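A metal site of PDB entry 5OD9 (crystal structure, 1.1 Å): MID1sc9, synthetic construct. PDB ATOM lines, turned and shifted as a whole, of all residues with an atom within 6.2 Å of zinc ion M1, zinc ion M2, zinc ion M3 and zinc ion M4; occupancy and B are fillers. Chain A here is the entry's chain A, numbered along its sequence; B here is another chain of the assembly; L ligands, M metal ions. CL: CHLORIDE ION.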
ATOM      1  N   GLN A  33      19.983 -15.391  20.517  1.00  0.00           N
ATOM      2  CA  GLN A  33      18.570 -14.967  20.544  1.00  0.00           C
ATOM      3  C   GLN A  33      18.049 -14.839  21.979  1.00  0.00           C
ATOM      4  O   GLN A  33      17.329 -13.895  22.311  1.00  0.00           O
ATOM      5  CB  GLN A  33      17.761 -15.934  19.732  1.00  0.00           C
ATOM      6  CG  GLN A  33      18.019 -15.830  18.199  1.00  0.00           C
ATOM      7  CD  GLN A  33      17.216 -16.830  17.402  1.00  0.00           C
ATOM      8  OE1 GLN A  33      16.935 -17.927  17.914  1.00  0.00           O
ATOM      9  NE2 GLN A  33      16.924 -16.551  16.154  1.00  0.00           N
ATOM     10  N   GLU A  34      18.407 -15.806  22.813  1.00  0.00           N
ATOM     11  CA  GLU A  34      17.876 -15.798  24.168  1.00  0.00           C
ATOM     12  C   GLU A  34      18.457 -14.648  24.972  1.00  0.00           C
ATOM     13  O   GLU A  34      17.749 -14.086  25.823  1.00  0.00           O
ATOM     14  CB  GLU A  34      18.156 -17.183  24.792  1.00  0.00           C
ATOM     15  CG  GLU A  34      17.282 -18.236  24.105  1.00  0.00           C
ATOM     16  CD  GLU A  34      17.514 -19.651  24.568  1.00  0.00           C
ATOM     17  OE1 GLU A  34      18.520 -19.922  25.201  1.00  0.00           O
ATOM     18  OE2 GLU A  34      16.640 -20.453  24.201  1.00  0.00           O
ATOM     19  N   HIS A  37      16.307 -11.731  23.784  1.00  0.00           N
ATOM     20  CA  HIS A  37      14.859 -11.806  24.117  1.00  0.00           C
ATOM     21  C   HIS A  37      14.353 -10.714  25.046  1.00  0.00           C
ATOM     22  O   HIS A  37      13.417  -9.988  24.637  1.00  0.00           O
ATOM     23  CB  HIS A  37      14.568 -13.233  24.604  1.00  0.00           C
ATOM     24  CG  HIS A  37      13.163 -13.544  24.941  1.00  0.00           C
ATOM     25  ND1 HIS A  37      12.370 -14.363  24.141  1.00  0.00           N
ATOM     26  CD2 HIS A  37      12.369 -13.147  25.982  1.00  0.00           C
ATOM     27  CE1 HIS A  37      11.196 -14.425  24.739  1.00  0.00           C
ATOM     28  NE2 HIS A  37      11.112 -13.696  25.861  1.00  0.00           N
ATOM     29  N   TRP A  40      14.872  -7.091  23.195  1.00  0.00           N
ATOM     30  CA  TRP A  40      13.911  -6.863  22.125  1.00  0.00           C
ATOM     31  C   TRP A  40      12.508  -6.664  22.658  1.00  0.00           C
ATOM     32  O   TRP A  40      11.787  -5.772  22.201  1.00  0.00           O
ATOM     33  CB  TRP A  40      13.945  -8.051  21.144  1.00  0.00           C
ATOM     34  CG  TRP A  40      12.795  -8.017  20.202  1.00  0.00           C
ATOM     35  CD1 TRP A  40      11.765  -8.933  20.171  1.00  0.00           C
ATOM     36  CD2 TRP A  40      12.498  -7.081  19.171  1.00  0.00           C
ATOM     37  NE1 TRP A  40      10.865  -8.614  19.208  1.00  0.00           N
ATOM     38  CE2 TRP A  40      11.290  -7.474  18.571  1.00  0.00           C
ATOM     39  CE3 TRP A  40      13.143  -5.903  18.678  1.00  0.00           C
ATOM     40  CZ2 TRP A  40      10.716  -6.773  17.536  1.00  0.00           C
ATOM     41  CZ3 TRP A  40      12.566  -5.216  17.648  1.00  0.00           C
ATOM     42  CH2 TRP A  40      11.378  -5.658  17.110  1.00  0.00           C
ATOM     43  N   HIS A  41      12.091  -7.425  23.653  1.00  0.00           N
ATOM     44  CA  HIS A  41      10.742  -7.188  24.167  1.00  0.00           C
ATOM     45  C   HIS A  41      10.591  -5.856  24.866  1.00  0.00           C
ATOM     46  O   HIS A  41       9.583  -5.185  24.682  1.00  0.00           O
ATOM     47  CB  HIS A  41      10.366  -8.345  25.086  1.00  0.00           C
ATOM     48  CG  HIS A  41       9.886  -9.517  24.271  1.00  0.00           C
ATOM     49  ND1 HIS A  41       9.690 -10.766  24.829  1.00  0.00           N
ATOM     50  CD2 HIS A  41       9.529  -9.617  22.964  1.00  0.00           C
ATOM     51  CE1 HIS A  41       9.257 -11.565  23.865  1.00  0.00           C
ATOM     52  NE2 HIS A  41       9.140 -10.950  22.719  1.00  0.00           N
ATOM     53  N   GLU A  60       8.168  -9.385  15.275  1.00  0.00           N
ATOM     54  CA  GLU A  60       7.760  -9.990  16.544  1.00  0.00           C
ATOM     55  C   GLU A  60       6.976 -11.275  16.341  1.00  0.00           C
ATOM     56  O   GLU A  60       7.156 -12.253  17.084  1.00  0.00           O
ATOM     57  CB  GLU A  60       7.023  -8.945  17.400  1.00  0.00           C
ATOM     58  CG  GLU A  60       6.414  -9.508  18.647  1.00  0.00           C
ATOM     59  CD  GLU A  60       7.333 -10.319  19.574  1.00  0.00           C
ATOM     60  OE1 GLU A  60       8.538 -10.123  19.546  1.00  0.00           O
ATOM     61  OE2 GLU A  60       6.833 -11.186  20.288  1.00  0.00           O
ATOM     62  N   HIS A  63       9.462 -13.942  15.875  1.00  0.00           N
ATOM     63  CA  HIS A  63       9.979 -14.343  17.150  1.00  0.00           C
ATOM     64  C   HIS A  63       9.055 -15.331  17.869  1.00  0.00           C
ATOM     65  O   HIS A  63       9.530 -16.333  18.365  1.00  0.00           O
ATOM     66  CB  HIS A  63      10.190 -13.057  17.996  1.00  0.00           C
ATOM     67  CG  HIS A  63      10.852 -13.365  19.323  1.00  0.00           C
ATOM     68  ND1 HIS A  63      10.458 -12.625  20.467  1.00  0.00           N
ATOM     69  CD2 HIS A  63      11.829 -14.208  19.685  1.00  0.00           C
ATOM     70  CE1 HIS A  63      11.254 -13.099  21.437  1.00  0.00           C
ATOM     71  NE2 HIS A  63      12.098 -14.044  21.039  1.00  0.00           N
ATOM     72  N   VAL A  64       7.775 -15.026  17.887  1.00  0.00           N
ATOM     73  CA  VAL A  64       6.813 -15.977  18.465  1.00  0.00           C
ATOM     74  C   VAL A  64       6.933 -17.309  17.754  1.00  0.00           C
ATOM     75  O   VAL A  64       6.945 -18.378  18.440  1.00  0.00           O
ATOM     76  CB  VAL A  64       5.391 -15.397  18.313  1.00  0.00           C
ATOM     77  CG1 VAL A  64       4.343 -16.443  18.597  1.00  0.00           C
ATOM     78  CG2 VAL A  64       5.204 -14.167  19.211  1.00  0.00           C
ATOM     79  N   HIS A  67       9.998 -19.358  18.713  1.00  0.00           N
ATOM     80  CA  HIS A  67       9.812 -20.092  19.929  1.00  0.00           C
ATOM     81  C   HIS A  67       9.021 -21.360  19.686  1.00  0.00           C
ATOM     82  O   HIS A  67       9.340 -22.428  20.194  1.00  0.00           O
ATOM     83  CB  HIS A  67       9.080 -19.254  20.991  1.00  0.00           C
ATOM     84  CG  HIS A  67       9.942 -18.360  21.779  1.00  0.00           C
ATOM     85  ND1 HIS A  67       9.991 -18.350  23.169  1.00  0.00           N
ATOM     86  CD2 HIS A  67      10.865 -17.470  21.366  1.00  0.00           C
ATOM     87  CE1 HIS A  67      10.902 -17.452  23.522  1.00  0.00           C
ATOM     88  NE2 HIS A  67      11.474 -16.880  22.468  1.00  0.00           N
ATOM     89  N   GLN A  68       7.999 -21.287  18.866  1.00  0.00           N
ATOM     90  CA  GLN A  68       7.162 -22.463  18.621  1.00  0.00           C
ATOM     91  C   GLN A  68       7.919 -23.538  17.838  1.00  0.00           C
ATOM     92  O   GLN A  68       7.812 -24.700  18.161  1.00  0.00           O
ATOM     93  CB  GLN A  68       5.853 -22.104  17.916  1.00  0.00           C
ATOM     94  CG  GLN A  68       4.996 -21.237  18.855  1.00  0.00           C
ATOM     95  CD  GLN A  68       4.134 -21.903  19.890  1.00  0.00           C
ATOM     96  OE1 GLN A  68       3.424 -22.884  19.652  1.00  0.00           O
ATOM     97  NE2 GLN A  68       4.090 -21.403  21.132  1.00  0.00           N
ATOM     98  N   ARG A  70      11.194 -23.932  17.759  1.00  0.00           N
ATOM     99  CA  ARG A  70      12.258 -24.480  18.618  1.00  0.00           C
ATOM    100  C   ARG A  70      11.605 -25.483  19.569  1.00  0.00           C
ATOM    101  O   ARG A  70      12.218 -26.552  19.769  1.00  0.00           O
ATOM    102  CB  ARG A  70      13.028 -23.341  19.321  1.00  0.00           C
ATOM    103  CG  ARG A  70      13.899 -23.632  20.507  1.00  0.00           C
ATOM    104  CD  ARG A  70      14.830 -22.408  20.761  1.00  0.00           C
ATOM    105  NE  ARG A  70      15.760 -22.110  19.675  1.00  0.00           N
ATOM    106  CZ  ARG A  70      16.005 -20.943  19.127  1.00  0.00           C
ATOM    107  NH1 ARG A  70      15.370 -19.859  19.587  1.00  0.00           N
ATOM    108  NH2 ARG A  70      16.895 -20.830  18.103  1.00  0.00           N
ATOM    109  N   GLN B  33      12.389 -12.165  34.995  1.00  0.00           N
ATOM    110  CA  GLN B  33      11.267 -12.958  34.574  1.00  0.00           C
ATOM    111  C   GLN B  33      11.390 -13.346  33.117  1.00  0.00           C
ATOM    112  O   GLN B  33      11.050 -14.440  32.675  1.00  0.00           O
ATOM    113  CB  GLN B  33       9.983 -12.126  34.749  1.00  0.00           C
ATOM    114  CG  GLN B  33       9.546 -12.034  36.207  1.00  0.00           C
ATOM    115  CD  GLN B  33       8.340 -11.136  36.432  1.00  0.00           C
ATOM    116  OE1 GLN B  33       7.869 -10.447  35.496  1.00  0.00           O
ATOM    117  NE2 GLN B  33       7.895 -11.203  37.689  1.00  0.00           N
ATOM    118  N   GLU B  34      11.891 -12.405  32.315  1.00  0.00           N
ATOM    119  CA  GLU B  34      12.120 -12.642  30.879  1.00  0.00           C
ATOM    120  C   GLU B  34      13.321 -13.529  30.642  1.00  0.00           C
ATOM    121  O   GLU B  34      13.263 -14.367  29.754  1.00  0.00           O
ATOM    122  CB  GLU B  34      12.161 -11.327  30.120  1.00  0.00           C
ATOM    123  CG  GLU B  34      10.747 -10.890  29.776  1.00  0.00           C
ATOM    124  CD  GLU B  34      10.204 -11.619  28.579  1.00  0.00           C
ATOM    125  OE1 GLU B  34       9.868 -12.833  28.756  1.00  0.00           O
ATOM    126  OE2 GLU B  34      10.203 -10.992  27.500  1.00  0.00           O
ATOM    127  N   HIS B  37      12.107 -17.145  30.861  1.00  0.00           N
ATOM    128  CA  HIS B  37      11.328 -17.731  29.772  1.00  0.00           C
ATOM    129  C   HIS B  37      12.179 -18.644  28.932  1.00  0.00           C
ATOM    130  O   HIS B  37      11.797 -19.832  28.851  1.00  0.00           O
ATOM    131  CB  HIS B  37      10.625 -16.525  29.120  1.00  0.00           C
ATOM    132  CG  HIS B  37       9.875 -16.823  27.874  1.00  0.00           C
ATOM    133  ND1 HIS B  37       9.298 -15.809  27.178  1.00  0.00           N
ATOM    134  CD2 HIS B  37       9.591 -17.954  27.198  1.00  0.00           C
ATOM    135  CE1 HIS B  37       8.688 -16.379  26.131  1.00  0.00           C
ATOM    136  NE2 HIS B  37       8.860 -17.689  26.092  1.00  0.00           N
ATOM    137  N   PRO B  38      13.198 -18.201  28.213  1.00  0.00           N
ATOM    138  CA  PRO B  38      13.955 -19.201  27.444  1.00  0.00           C
ATOM    139  C   PRO B  38      14.566 -20.283  28.319  1.00  0.00           C
ATOM    140  O   PRO B  38      14.724 -21.401  27.869  1.00  0.00           O
ATOM    141  CB  PRO B  38      15.041 -18.420  26.718  1.00  0.00           C
ATOM    142  CG  PRO B  38      14.755 -16.988  26.947  1.00  0.00           C
ATOM    143  CD  PRO B  38      13.691 -16.864  27.970  1.00  0.00           C
ATOM    144  N   HIS B  41      12.034 -22.954  28.793  1.00  0.00           N
ATOM    145  CA  HIS B  41      11.863 -23.788  27.617  1.00  0.00           C
ATOM    146  C   HIS B  41      13.000 -24.783  27.451  1.00  0.00           C
ATOM    147  O   HIS B  41      12.746 -25.919  27.061  1.00  0.00           O
ATOM    148  CB  HIS B  41      11.796 -22.938  26.346  1.00  0.00           C
ATOM    149  CG  HIS B  41      10.567 -22.175  26.079  1.00  0.00           C
ATOM    150  ND1 HIS B  41       9.282 -22.571  26.370  1.00  0.00           N
ATOM    151  CD2 HIS B  41      10.406 -20.965  25.472  1.00  0.00           C
ATOM    152  CE1 HIS B  41       8.437 -21.695  25.955  1.00  0.00           C
ATOM    153  NE2 HIS B  41       9.080 -20.678  25.382  1.00  0.00           N
ATOM    154  N   HIS B  63       4.241 -19.583  29.420  1.00  0.00           N
ATOM    155  CA  HIS B  63       5.193 -18.808  28.616  1.00  0.00           C
ATOM    156  C   HIS B  63       4.721 -18.568  27.200  1.00  0.00           C
ATOM    157  O   HIS B  63       4.865 -17.454  26.706  1.00  0.00           O
ATOM    158  CB  HIS B  63       6.558 -19.470  28.627  1.00  0.00           C
ATOM    159  CG  HIS B  63       7.205 -19.369  29.973  1.00  0.00           C
ATOM    160  ND1 HIS B  63       7.755 -18.247  30.485  1.00  0.00           N
ATOM    161  CD2 HIS B  63       7.307 -20.331  30.904  1.00  0.00           C
ATOM    162  CE1 HIS B  63       8.217 -18.495  31.713  1.00  0.00           C
ATOM    163  NE2 HIS B  63       7.959 -19.772  32.025  1.00  0.00           N
ATOM    164  N   VAL B  64       4.149 -19.560  26.555  1.00  0.00           N
ATOM    165  CA  VAL B  64       3.568 -19.390  25.204  1.00  0.00           C
ATOM    166  C   VAL B  64       2.566 -18.238  25.204  1.00  0.00           C
ATOM    167  O   VAL B  64       2.564 -17.389  24.325  1.00  0.00           O
ATOM    168  CB  VAL B  64       2.960 -20.706  24.659  1.00  0.00           C
ATOM    169  CG1 VAL B  64       2.158 -20.451  23.412  1.00  0.00           C
ATOM    170  CG2 VAL B  64       4.021 -21.756  24.452  1.00  0.00           C
ATOM    171  N   ILE B  66       2.125 -15.799  27.541  1.00  0.00           N
ATOM    172  CA  ILE B  66       2.784 -14.509  27.840  1.00  0.00           C
ATOM    173  C   ILE B  66       3.325 -13.930  26.543  1.00  0.00           C
ATOM    174  O   ILE B  66       3.146 -12.744  26.272  1.00  0.00           O
ATOM    175  CB  ILE B  66       3.849 -14.654  28.875  1.00  0.00           C
ATOM    176  CG1 ILE B  66       3.301 -15.035  30.267  1.00  0.00           C
ATOM    177  CG2 ILE B  66       4.709 -13.402  28.966  1.00  0.00           C
ATOM    178  CD1 ILE B  66       4.302 -15.634  31.185  1.00  0.00           C
ATOM    179  N   HIS B  67       4.011 -14.757  25.752  1.00  0.00           N
ATOM    180  CA  HIS B  67       4.631 -14.243  24.547  1.00  0.00           C
ATOM    181  C   HIS B  67       3.577 -13.716  23.553  1.00  0.00           C
ATOM    182  O   HIS B  67       3.742 -12.631  22.974  1.00  0.00           O
ATOM    183  CB  HIS B  67       5.492 -15.350  23.909  1.00  0.00           C
ATOM    184  CG  HIS B  67       6.508 -14.800  22.943  1.00  0.00           C
ATOM    185  ND1 HIS B  67       7.495 -15.588  22.400  1.00  0.00           N
ATOM    186  CD2 HIS B  67       6.764 -13.571  22.486  1.00  0.00           C
ATOM    187  CE1 HIS B  67       8.285 -14.848  21.650  1.00  0.00           C
ATOM    188  NE2 HIS B  67       7.879 -13.602  21.693  1.00  0.00           N
ATOM    189  N   ARG B  70       2.278 -10.443  24.769  1.00  0.00           N
ATOM    190  CA  ARG B  70       3.198  -9.345  24.561  1.00  0.00           C
ATOM    191  C   ARG B  70       3.229  -8.879  23.110  1.00  0.00           C
ATOM    192  O   ARG B  70       3.261  -7.720  22.806  1.00  0.00           O
ATOM    193  CB  ARG B  70       4.585  -9.758  25.099  1.00  0.00           C
ATOM    194  CG  ARG B  70       5.440  -8.536  25.372  1.00  0.00           C
ATOM    195  CD  ARG B  70       6.874  -8.944  25.721  1.00  0.00           C
ATOM    196  NE  ARG B  70       6.945  -9.982  26.741  1.00  0.00           N
ATOM    197  CZ  ARG B  70       6.993  -9.802  28.055  1.00  0.00           C
ATOM    198  NH1 ARG B  70       6.974  -8.617  28.565  1.00  0.00           N
ATOM    199  NH2 ARG B  70       7.066 -10.893  28.812  1.00  0.00           N
ATOM    200  N   ALA B  71       3.168  -9.856  22.196  1.00  0.00           N
ATOM    201  CA  ALA B  71       3.222  -9.539  20.767  1.00  0.00           C
ATOM    202  C   ALA B  71       1.996  -8.704  20.369  1.00  0.00           C
ATOM    203  O   ALA B  71       2.084  -7.908  19.452  1.00  0.00           O
ATOM    204  CB  ALA B  71       3.268 -10.817  19.920  1.00  0.00           C
HETATM  205 CL    CL L   1      14.818 -16.114  22.104  1.00  0.00          CL
HETATM  206 CL    CL L   2       6.673 -18.713  23.455  1.00  0.00          CL
HETATM  207 CL    CL L   3       7.541 -13.204  26.244  1.00  0.00          CL
HETATM  208 ZN    ZN M   1      12.772 -15.332  22.434  1.00  0.00          ZN
HETATM  209 ZN    ZN M   2       8.704 -11.850  20.979  1.00  0.00          ZN
HETATM  210 ZN    ZN M   3       8.603 -18.916  24.524  1.00  0.00          ZN
HETATM  211 ZN    ZN M   4       9.549 -13.814  27.102  1.00  0.00          ZN
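NE2 of His 37 of chain A lies close to ND1 of His 41 of chain A, 3.4 Å away.
ND1 of His 41 of chain A lies within hydrogen-bond range of OE2 of Glu 34 of chain B (2.7 Å).
NE1 of Trp 40 lies close to OE1 of Glu 60 (2.8 Å).
The guanidinium group (NH2) of Arg 70 of chain B is in salt-bridge range of the side-chain carboxylate (OE2) of Glu 34 of chain B (3.4 Å).
ND1 of His 41 of chain A is in hydrogen-bond range of NE of Arg 70 of chain B (3.4 Å).
The nearest printed residue that does not touch zinc ion M1 is His 67 of chain B (4.6 Å).
Of the 22 residues printed, 4 come within 4 Å of zinc ion M2.
Of the 22 residues printed, 3 come within 4 Å of zinc ion M3.
Four residues have an atom within 4 Å of zinc ion M4: His 37 of chain A, His 41 of chain A, Glu 34 of chain B and His 37 of chain B.
Zinc ion M1 is bound by ND1 of His 37 of chain A (2.0 Å), NE2 of His 63 of chain A (2.0 Å), NE2 of His 67 of chain A (2.0 Å) and CL of CL L1 (2.2 Å).
Zinc ion M2 is bound by ND1 of His 63 of chain A (2.0 Å), NE2 of His 41 of chain A (2.0 Å), NE2 of His 67 of chain B (2.1 Å), OE2 of Glu 60 (2.1 Å) and OE1 of Glu 60 (2.3 Å).
Zinc ion M3 is bound by NE2 of His 37 of chain B (2.0 Å), NE2 of His 41 of chain B (2.0 Å), ND1 of His 67 of chain A (2.0 Å) and CL of CL L2 (2.2 Å).
Zinc ion M3 has four donor atoms within binding distance.
Zinc ion M4 is bound by OE1 of Glu 34 of chain B, NE2 of His 37 of chain A, ND1 of His 37 of chain B and CL of CL L3.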
